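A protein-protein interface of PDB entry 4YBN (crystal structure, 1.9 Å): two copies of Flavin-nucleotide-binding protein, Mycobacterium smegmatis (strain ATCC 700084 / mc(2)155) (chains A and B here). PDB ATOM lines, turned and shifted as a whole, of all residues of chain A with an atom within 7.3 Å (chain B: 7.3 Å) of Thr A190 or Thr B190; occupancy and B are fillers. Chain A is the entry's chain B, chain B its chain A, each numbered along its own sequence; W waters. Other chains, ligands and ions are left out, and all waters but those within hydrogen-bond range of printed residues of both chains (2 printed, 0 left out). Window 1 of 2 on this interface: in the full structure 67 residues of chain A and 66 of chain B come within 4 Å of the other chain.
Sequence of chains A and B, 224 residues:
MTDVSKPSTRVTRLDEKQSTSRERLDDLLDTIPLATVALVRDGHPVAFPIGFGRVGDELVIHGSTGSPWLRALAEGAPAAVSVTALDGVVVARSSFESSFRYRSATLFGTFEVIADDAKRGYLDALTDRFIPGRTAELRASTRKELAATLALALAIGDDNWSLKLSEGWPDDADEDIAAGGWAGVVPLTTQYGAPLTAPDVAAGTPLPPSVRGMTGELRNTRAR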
ATOM      1  N   ILE A  32      -2.997  10.725  -7.805  1.00  0.00           N
ATOM      2  CA  ILE A  32      -1.711  10.197  -7.368  1.00  0.00           C
ATOM      3  C   ILE A  32      -0.745  10.388  -8.495  1.00  0.00           C
ATOM      4  O   ILE A  32      -1.042   9.913  -9.582  1.00  0.00           O
ATOM      5  CB  ILE A  32      -1.795   8.654  -7.135  1.00  0.00           C
ATOM      6  CG1 ILE A  32      -2.724   8.304  -5.937  1.00  0.00           C
ATOM      7  CG2 ILE A  32      -0.428   8.076  -6.850  1.00  0.00           C
ATOM      8  CD1 ILE A  32      -2.273   8.923  -4.610  1.00  0.00           C
ATOM      9  N   LEU A  86      -3.107   5.241  -0.544  1.00  0.00           N
ATOM     10  CA  LEU A  86      -3.383   4.717   0.793  1.00  0.00           C
ATOM     11  C   LEU A  86      -4.311   5.717   1.505  1.00  0.00           C
ATOM     12  O   LEU A  86      -3.948   6.850   1.697  1.00  0.00           O
ATOM     13  CB  LEU A  86      -2.078   4.638   1.490  1.00  0.00           C
ATOM     14  CG  LEU A  86      -2.157   4.168   2.912  1.00  0.00           C
ATOM     15  CD1 LEU A  86      -2.843   2.827   3.037  1.00  0.00           C
ATOM     16  CD2 LEU A  86      -0.713   4.106   3.411  1.00  0.00           C
ATOM     17  N   LEU A 188      -5.842   8.379   6.447  1.00  0.00           N
ATOM     18  CA  LEU A 188      -4.593   8.923   6.023  1.00  0.00           C
ATOM     19  C   LEU A 188      -4.852   9.886   4.838  1.00  0.00           C
ATOM     20  O   LEU A 188      -5.628   9.574   3.926  1.00  0.00           O
ATOM     21  CB  LEU A 188      -3.700   7.783   5.581  1.00  0.00           C
ATOM     22  CG  LEU A 188      -3.187   6.969   6.728  1.00  0.00           C
ATOM     23  CD1 LEU A 188      -2.809   5.588   6.259  1.00  0.00           C
ATOM     24  CD2 LEU A 188      -2.037   7.708   7.361  1.00  0.00           C
ATOM     25  N   THR A 189      -4.197  11.034   4.858  1.00  0.00           N
ATOM     26  CA  THR A 189      -4.296  11.957   3.709  1.00  0.00           C
ATOM     27  C   THR A 189      -2.908  12.476   3.400  1.00  0.00           C
ATOM     28  O   THR A 189      -2.000  12.562   4.284  1.00  0.00           O
ATOM     29  CB  THR A 189      -5.205  13.176   4.010  1.00  0.00           C
ATOM     30  OG1 THR A 189      -4.606  13.904   5.075  1.00  0.00           O
ATOM     31  CG2 THR A 189      -6.601  12.756   4.418  1.00  0.00           C
ATOM     32  N   THR A 190      -2.726  12.805   2.144  1.00  0.00           N
ATOM     33  CA  THR A 190      -1.465  13.427   1.736  1.00  0.00           C
ATOM     34  C   THR A 190      -1.721  14.882   1.374  1.00  0.00           C
ATOM     35  O   THR A 190      -2.632  15.148   0.640  1.00  0.00           O
ATOM     36  CB  THR A 190      -0.890  12.662   0.560  1.00  0.00           C
ATOM     37  OG1 THR A 190      -0.757  11.324   1.000  1.00  0.00           O
ATOM     38  CG2 THR A 190       0.516  13.209   0.215  1.00  0.00           C
ATOM     39  N   GLN A 191      -0.919  15.788   1.920  1.00  0.00           N
ATOM     40  CA  GLN A 191      -1.218  17.206   1.854  1.00  0.00           C
ATOM     41  C   GLN A 191       0.026  17.950   1.379  1.00  0.00           C
ATOM     42  O   GLN A 191       1.105  17.598   1.749  1.00  0.00           O
ATOM     43  CB  GLN A 191      -1.563  17.711   3.258  1.00  0.00           C
ATOM     44  CG  GLN A 191      -2.596  16.908   4.033  1.00  0.00           C
ATOM     45  CD  GLN A 191      -3.997  17.403   3.759  1.00  0.00           C
ATOM     46  OE1 GLN A 191      -4.193  18.569   3.395  1.00  0.00           O
ATOM     47  NE2 GLN A 191      -4.980  16.525   3.916  1.00  0.00           N
ATOM     48  N   TYR A 192      -0.156  18.966   0.551  1.00  0.00           N
ATOM     49  CA  TYR A 192       0.910  19.891   0.238  1.00  0.00           C
ATOM     50  C   TYR A 192       1.187  20.730   1.467  1.00  0.00           C
ATOM     51  O   TYR A 192       0.272  21.155   2.134  1.00  0.00           O
ATOM     52  CB  TYR A 192       0.450  20.855  -0.862  1.00  0.00           C
ATOM     53  CG  TYR A 192       0.218  20.267  -2.202  1.00  0.00           C
ATOM     54  CD1 TYR A 192       1.262  19.826  -2.954  1.00  0.00           C
ATOM     55  CD2 TYR A 192      -1.052  20.213  -2.740  1.00  0.00           C
ATOM     56  CE1 TYR A 192       1.068  19.332  -4.206  1.00  0.00           C
ATOM     57  CE2 TYR A 192      -1.265  19.708  -3.982  1.00  0.00           C
ATOM     58  CZ  TYR A 192      -0.180  19.291  -4.714  1.00  0.00           C
ATOM     59  OH  TYR A 192      -0.370  18.752  -5.948  1.00  0.00           O
ATOM     60  N   GLY A 216      -3.765  22.186   0.249  1.00  0.00           N
ATOM     61  CA  GLY A 216      -4.726  21.101   0.555  1.00  0.00           C
ATOM     62  C   GLY A 216      -4.203  19.736   0.097  1.00  0.00           C
ATOM     63  O   GLY A 216      -3.005  19.539  -0.024  1.00  0.00           O
ATOM     64  N   GLU A 217      -5.111  18.810  -0.199  1.00  0.00           N
ATOM     65  CA  GLU A 217      -4.714  17.436  -0.478  1.00  0.00           C
ATOM     66  C   GLU A 217      -4.063  17.299  -1.829  1.00  0.00           C
ATOM     67  O   GLU A 217      -4.391  18.021  -2.751  1.00  0.00           O
ATOM     68  CB  GLU A 217      -5.912  16.513  -0.466  1.00  0.00           C
ATOM     69  CG  GLU A 217      -6.534  16.356   0.849  1.00  0.00           C
ATOM     70  CD  GLU A 217      -7.368  15.082   0.919  1.00  0.00           C
ATOM     71  OE1 GLU A 217      -8.098  14.887   1.901  1.00  0.00           O
ATOM     72  OE2 GLU A 217      -7.293  14.236   0.007  1.00  0.00           O
ATOM     73  N   LEU A 218      -3.112  16.407  -1.966  1.00  0.00           N
ATOM     74  CA  LEU A 218      -2.765  15.960  -3.304  1.00  0.00           C
ATOM     75  C   LEU A 218      -4.139  15.627  -3.885  1.00  0.00           C
ATOM     76  O   LEU A 218      -4.838  14.799  -3.323  1.00  0.00           O
ATOM     77  CB  LEU A 218      -1.958  14.705  -3.239  1.00  0.00           C
ATOM     78  CG  LEU A 218      -0.531  14.656  -3.699  1.00  0.00           C
ATOM     79  CD1 LEU A 218      -0.124  13.184  -3.717  1.00  0.00           C
ATOM     80  CD2 LEU A 218      -0.338  15.299  -5.050  1.00  0.00           C
ATOM     81  N   ARG A 219      -4.571  16.297  -4.948  1.00  0.00           N
ATOM     82  CA  ARG A 219      -6.035  16.373  -5.246  1.00  0.00           C
ATOM     83  C   ARG A 219      -6.336  16.196  -6.732  1.00  0.00           C
ATOM     84  O   ARG A 219      -5.489  16.475  -7.575  1.00  0.00           O
ATOM     85  CB  ARG A 219      -6.584  17.744  -4.788  1.00  0.00           C
ATOM     86  CG  ARG A 219      -7.942  17.736  -4.104  1.00  0.00           C
ATOM     87  CD  ARG A 219      -8.255  19.107  -3.504  1.00  0.00           C
ATOM     88  NE  ARG A 219      -9.683  19.408  -3.570  1.00  0.00           N
ATOM     89  CZ  ARG A 219     -10.335  19.737  -4.684  1.00  0.00           C
ATOM     90  NH1 ARG A 219      -9.700  19.812  -5.851  1.00  0.00           N
ATOM     91  NH2 ARG A 219     -11.634  19.991  -4.636  1.00  0.00           N
ATOM     92  N   ILE B  32       6.963   3.826   5.595  1.00  0.00           N
ATOM     93  CA  ILE B  32       5.899   3.585   4.607  1.00  0.00           C
ATOM     94  C   ILE B  32       5.390   2.198   4.802  1.00  0.00           C
ATOM     95  O   ILE B  32       6.195   1.300   4.773  1.00  0.00           O
ATOM     96  CB  ILE B  32       6.493   3.699   3.168  1.00  0.00           C
ATOM     97  CG1 ILE B  32       7.146   5.087   2.970  1.00  0.00           C
ATOM     98  CG2 ILE B  32       5.418   3.474   2.107  1.00  0.00           C
ATOM     99  CD1 ILE B  32       6.151   6.221   3.046  1.00  0.00           C
ATOM    100  N   PRO B  33       4.075   1.987   4.963  1.00  0.00           N
ATOM    101  CA  PRO B  33       3.538   0.648   5.151  1.00  0.00           C
ATOM    102  C   PRO B  33       3.132  -0.110   3.877  1.00  0.00           C
ATOM    103  O   PRO B  33       2.759  -1.264   3.958  1.00  0.00           O
ATOM    104  CB  PRO B  33       2.312   0.912   5.998  1.00  0.00           C
ATOM    105  CG  PRO B  33       1.829   2.186   5.514  1.00  0.00           C
ATOM    106  CD  PRO B  33       3.024   3.006   5.145  1.00  0.00           C
ATOM    107  N   LEU B  86       6.928   9.694  -1.317  1.00  0.00           N
ATOM    108  CA  LEU B  86       6.889  10.953  -2.101  1.00  0.00           C
ATOM    109  C   LEU B  86       6.861  12.106  -1.146  1.00  0.00           C
ATOM    110  O   LEU B  86       5.890  12.236  -0.414  1.00  0.00           O
ATOM    111  CB  LEU B  86       5.608  10.973  -2.909  1.00  0.00           C
ATOM    112  CG  LEU B  86       5.284  12.174  -3.834  1.00  0.00           C
ATOM    113  CD1 LEU B  86       6.431  12.434  -4.748  1.00  0.00           C
ATOM    114  CD2 LEU B  86       4.040  11.886  -4.644  1.00  0.00           C
ATOM    115  N   PRO B 187       6.387  20.814  -0.344  1.00  0.00           N
ATOM    116  CA  PRO B 187       6.465  19.528   0.349  1.00  0.00           C
ATOM    117  C   PRO B 187       5.174  18.760   0.321  1.00  0.00           C
ATOM    118  O   PRO B 187       4.089  19.355   0.172  1.00  0.00           O
ATOM    119  CB  PRO B 187       6.718  19.937   1.799  1.00  0.00           C
ATOM    120  CG  PRO B 187       7.286  21.303   1.704  1.00  0.00           C
ATOM    121  CD  PRO B 187       6.483  21.920   0.624  1.00  0.00           C
ATOM    122  N   LEU B 188       5.330  17.452   0.485  1.00  0.00           N
ATOM    123  CA  LEU B 188       4.210  16.510   0.621  1.00  0.00           C
ATOM    124  C   LEU B 188       4.431  15.695   1.877  1.00  0.00           C
ATOM    125  O   LEU B 188       5.530  15.223   2.148  1.00  0.00           O
ATOM    126  CB  LEU B 188       4.111  15.606  -0.591  1.00  0.00           C
ATOM    127  CG  LEU B 188       3.563  16.298  -1.846  1.00  0.00           C
ATOM    128  CD1 LEU B 188       3.949  15.626  -3.150  1.00  0.00           C
ATOM    129  CD2 LEU B 188       2.052  16.467  -1.788  1.00  0.00           C
ATOM    130  N   THR B 189       3.367  15.589   2.679  1.00  0.00           N
ATOM    131  CA  THR B 189       3.393  14.755   3.871  1.00  0.00           C
ATOM    132  C   THR B 189       2.111  13.940   3.929  1.00  0.00           C
ATOM    133  O   THR B 189       1.080  14.336   3.411  1.00  0.00           O
ATOM    134  CB  THR B 189       3.498  15.568   5.157  1.00  0.00           C
ATOM    135  OG1 THR B 189       2.372  16.429   5.261  1.00  0.00           O
ATOM    136  CG2 THR B 189       4.735  16.454   5.149  1.00  0.00           C
ATOM    137  N   THR B 190       2.216  12.792   4.577  1.00  0.00           N
ATOM    138  CA  THR B 190       1.106  11.910   4.745  1.00  0.00           C
ATOM    139  C   THR B 190       0.877  11.851   6.209  1.00  0.00           C
ATOM    140  O   THR B 190       1.799  11.623   6.978  1.00  0.00           O
ATOM    141  CB  THR B 190       1.393  10.566   4.075  1.00  0.00           C
ATOM    142  OG1 THR B 190       1.398  10.785   2.656  1.00  0.00           O
ATOM    143  CG2 THR B 190       0.297   9.562   4.387  1.00  0.00           C
ATOM    144  N   GLN B 191      -0.369  12.134   6.607  1.00  0.00           N
ATOM    145  CA  GLN B 191      -0.733  12.268   7.987  1.00  0.00           C
ATOM    146  C   GLN B 191      -1.985  11.485   8.367  1.00  0.00           C
ATOM    147  O   GLN B 191      -2.900  11.377   7.567  1.00  0.00           O
ATOM    148  CB  GLN B 191      -0.962  13.737   8.298  1.00  0.00           C
ATOM    149  CG  GLN B 191       0.136  14.272   9.202  1.00  0.00           C
ATOM    150  CD  GLN B 191       0.218  15.765   9.080  1.00  0.00           C
ATOM    151  OE1 GLN B 191       0.777  16.287   8.107  1.00  0.00           O
ATOM    152  NE2 GLN B 191      -0.367  16.474  10.061  1.00  0.00           N
ATOM    153  N   TYR B 192      -2.015  11.032   9.611  1.00  0.00           N
ATOM    154  CA  TYR B 192      -3.184  10.401  10.189  1.00  0.00           C
ATOM    155  C   TYR B 192      -4.245  11.488  10.511  1.00  0.00           C
ATOM    156  O   TYR B 192      -3.912  12.501  11.064  1.00  0.00           O
ATOM    157  CB  TYR B 192      -2.832   9.701  11.484  1.00  0.00           C
ATOM    158  CG  TYR B 192      -1.915   8.507  11.395  1.00  0.00           C
ATOM    159  CD1 TYR B 192      -2.351   7.336  10.844  1.00  0.00           C
ATOM    160  CD2 TYR B 192      -0.587   8.590  11.859  1.00  0.00           C
ATOM    161  CE1 TYR B 192      -1.511   6.247  10.743  1.00  0.00           C
ATOM    162  CE2 TYR B 192       0.242   7.520  11.774  1.00  0.00           C
ATOM    163  CZ  TYR B 192      -0.230   6.351  11.215  1.00  0.00           C
ATOM    164  OH  TYR B 192       0.640   5.262  11.133  1.00  0.00           O
ATOM    165  N   GLY B 216       0.204  12.360  13.817  1.00  0.00           N
ATOM    166  CA  GLY B 216       1.364  12.926  13.108  1.00  0.00           C
ATOM    167  C   GLY B 216       1.514  12.288  11.745  1.00  0.00           C
ATOM    168  O   GLY B 216       0.561  11.736  11.153  1.00  0.00           O
ATOM    169  N   GLU B 217       2.750  12.272  11.296  1.00  0.00           N
ATOM    170  CA  GLU B 217       3.063  11.732  10.014  1.00  0.00           C
ATOM    171  C   GLU B 217       3.167  10.233  10.063  1.00  0.00           C
ATOM    172  O   GLU B 217       3.718   9.614  10.960  1.00  0.00           O
ATOM    173  CB  GLU B 217       4.345  12.322   9.459  1.00  0.00           C
ATOM    174  CG  GLU B 217       4.223  13.790   9.128  1.00  0.00           C
ATOM    175  CD  GLU B 217       5.515  14.373   8.571  1.00  0.00           C
ATOM    176  OE1 GLU B 217       6.444  13.623   8.201  1.00  0.00           O
ATOM    177  OE2 GLU B 217       5.593  15.600   8.496  1.00  0.00           O
ATOM    178  N   LEU B 218       2.591   9.666   9.049  1.00  0.00           N
ATOM    179  CA  LEU B 218       2.479   8.245   8.879  1.00  0.00           C
ATOM    180  C   LEU B 218       3.815   7.601   9.104  1.00  0.00           C
ATOM    181  O   LEU B 218       4.771   8.050   8.488  1.00  0.00           O
ATOM    182  CB  LEU B 218       2.076   7.994   7.434  1.00  0.00           C
ATOM    183  CG  LEU B 218       2.418   6.649   6.851  1.00  0.00           C
ATOM    184  CD1 LEU B 218       1.453   5.640   7.466  1.00  0.00           C
ATOM    185  CD2 LEU B 218       2.432   6.702   5.324  1.00  0.00           C
ATOM    186  N   ARG B 219       3.877   6.570   9.980  1.00  0.00           N
ATOM    187  CA  ARG B 219       5.087   5.706  10.114  1.00  0.00           C
ATOM    188  C   ARG B 219       4.732   4.188  10.110  1.00  0.00           C
ATOM    189  O   ARG B 219       3.558   3.814  10.121  1.00  0.00           O
ATOM    190  CB  ARG B 219       6.005   6.141  11.298  1.00  0.00           C
ATOM    191  CG  ARG B 219       6.897   7.326  10.901  1.00  0.00           C
ATOM    192  CD  ARG B 219       8.167   7.445  11.702  1.00  0.00           C
ATOM    193  NE  ARG B 219       9.211   6.420  11.499  1.00  0.00           N
ATOM    194  CZ  ARG B 219       9.958   5.927  12.491  1.00  0.00           C
ATOM    195  NH1 ARG B 219       9.715   6.299  13.746  1.00  0.00           N
ATOM    196  NH2 ARG B 219      10.921   5.028  12.255  1.00  0.00           N
HETATM  197  O   HOH W   1       2.349  18.665   3.988  1.00  0.00           O
HETATM  198  O   HOH W   2      -5.202  12.906   7.324  1.00  0.00           O
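Leu A86 touches Pro B33 (CD2 to CG, 3.8 Å). CA of Leu A188 touches O of Gln B191 (3.4 Å). Tyr B192 touches Leu A188. O of Thr A189 touches O of Thr B189, at 3.7 Å. Thr A189 touches Thr B190. Thr A190 touches Thr B189 (CA to O, 3.2 Å). Pro B187 touches Gln A191 (O to O, 3.8 Å). Gln A191 touches Leu B188 (O to CA, 3.5 Å). Pro B187 touches Tyr A192 (O to CA, 3.2 Å). Leu B188 touches Leu A218 (CD2 to CG, 3.7 Å).
O of Thr B190 sits at hydrogen-bond distance from N of Leu B218, at 3.0 Å. The backbone NH (N) of Tyr B192 sits at hydrogen-bond distance from the backbone carbonyl oxygen (O) of Gly B216 (3.1 Å). The side-chain hydroxyl (OH) of Tyr B192 sits at hydrogen-bond distance from the backbone carbonyl oxygen (O) of Arg B219 (3.4 Å). OG1 of Thr A189 sits at hydrogen-bond distance from NE2 of Gln A191, 2.9 Å away. The backbone carbonyl oxygen (O) of Thr A190 is in hydrogen-bond range of the backbone NH (N) of Leu A218 (2.9 Å). N of Tyr A192 is in hydrogen-bond range of O of Gly A216 (3.0 Å).
Water W2 bridges OG1 of Thr A189 (2.5 Å) and O of Gln B191 (2.8 Å). Water W1 lies within hydrogen-bond range of OG1 of Thr B189 (2.6 Å) and O of Gln A191 (2.8 Å).
Of the 13 printed residues of chain B, 7 touch a printed residue of chain A. Printed residues of chain B that touch a printed residue of chain A: Pro B33, Pro B187, Leu B188, Thr B189, Thr B190, Gln B191 and Tyr B192. Hydrophobic or aromatic side chains of chain B within 4 Å of the printed part of chain A: Pro B33, Leu B188 and Tyr B192. Hydrophobic or aromatic side chains of chain A within 4 Å of the printed part of chain B: Leu A86, Leu A188, Tyr A192 and Leu A218.
O of Thr B189 lies within hydrogen-bond range of N of Gln A191 (2.9 Å). The side-chain hydroxyl of Thr A190 sits at hydrogen-bond distance from the side-chain hydroxyl of Thr B190 (2.8 Å). The backbone NH (N) of Gln B191 lies within hydrogen-bond range of the backbone carbonyl oxygen (O) of Thr A189, at 2.9 Å.
Leu A188 touches Gln B191, and with the chains exchanged Gln A191 touches Leu B188. Leu A188 touches Tyr B192, and with the chains exchanged Tyr A192 touches Leu B188. Thr B189 touches its own counterpart, Thr A189. Leu A218 touches Leu B188, but with the chains exchanged Leu A188 does not touch Leu B218 (4.1 Å). 11 positions are printed for both chains.
Thr A190 touches just these residues of chain B: Thr B189 (3.2 Å) and Thr B190 (2.8 Å). Printed residues of chain A within 4 Å of Thr B190: Thr A189 (3.2 Å) and Thr A190 (2.8 Å). Printed residues of chain B within 4 Å of Leu A86: Pro B33. Of the printed residues of chain A, Gln B191 touches Leu A188 and Thr A189. Of the printed residues of chain B, Leu A188 touches Gln B191 (3.4 Å) and Tyr B192 (3.5 Å). Ile A32 touches none of the printed residues of chain B. The nearest residue of chain B that does not touch Thr A190 is Leu B188 (4.1 Å). The nearest residue of chain A that does not touch Thr B190 is Leu A188 (4.2 Å). The nearest printed residue of chain B that does not touch Tyr A192 is Thr B189 (5.3 Å).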
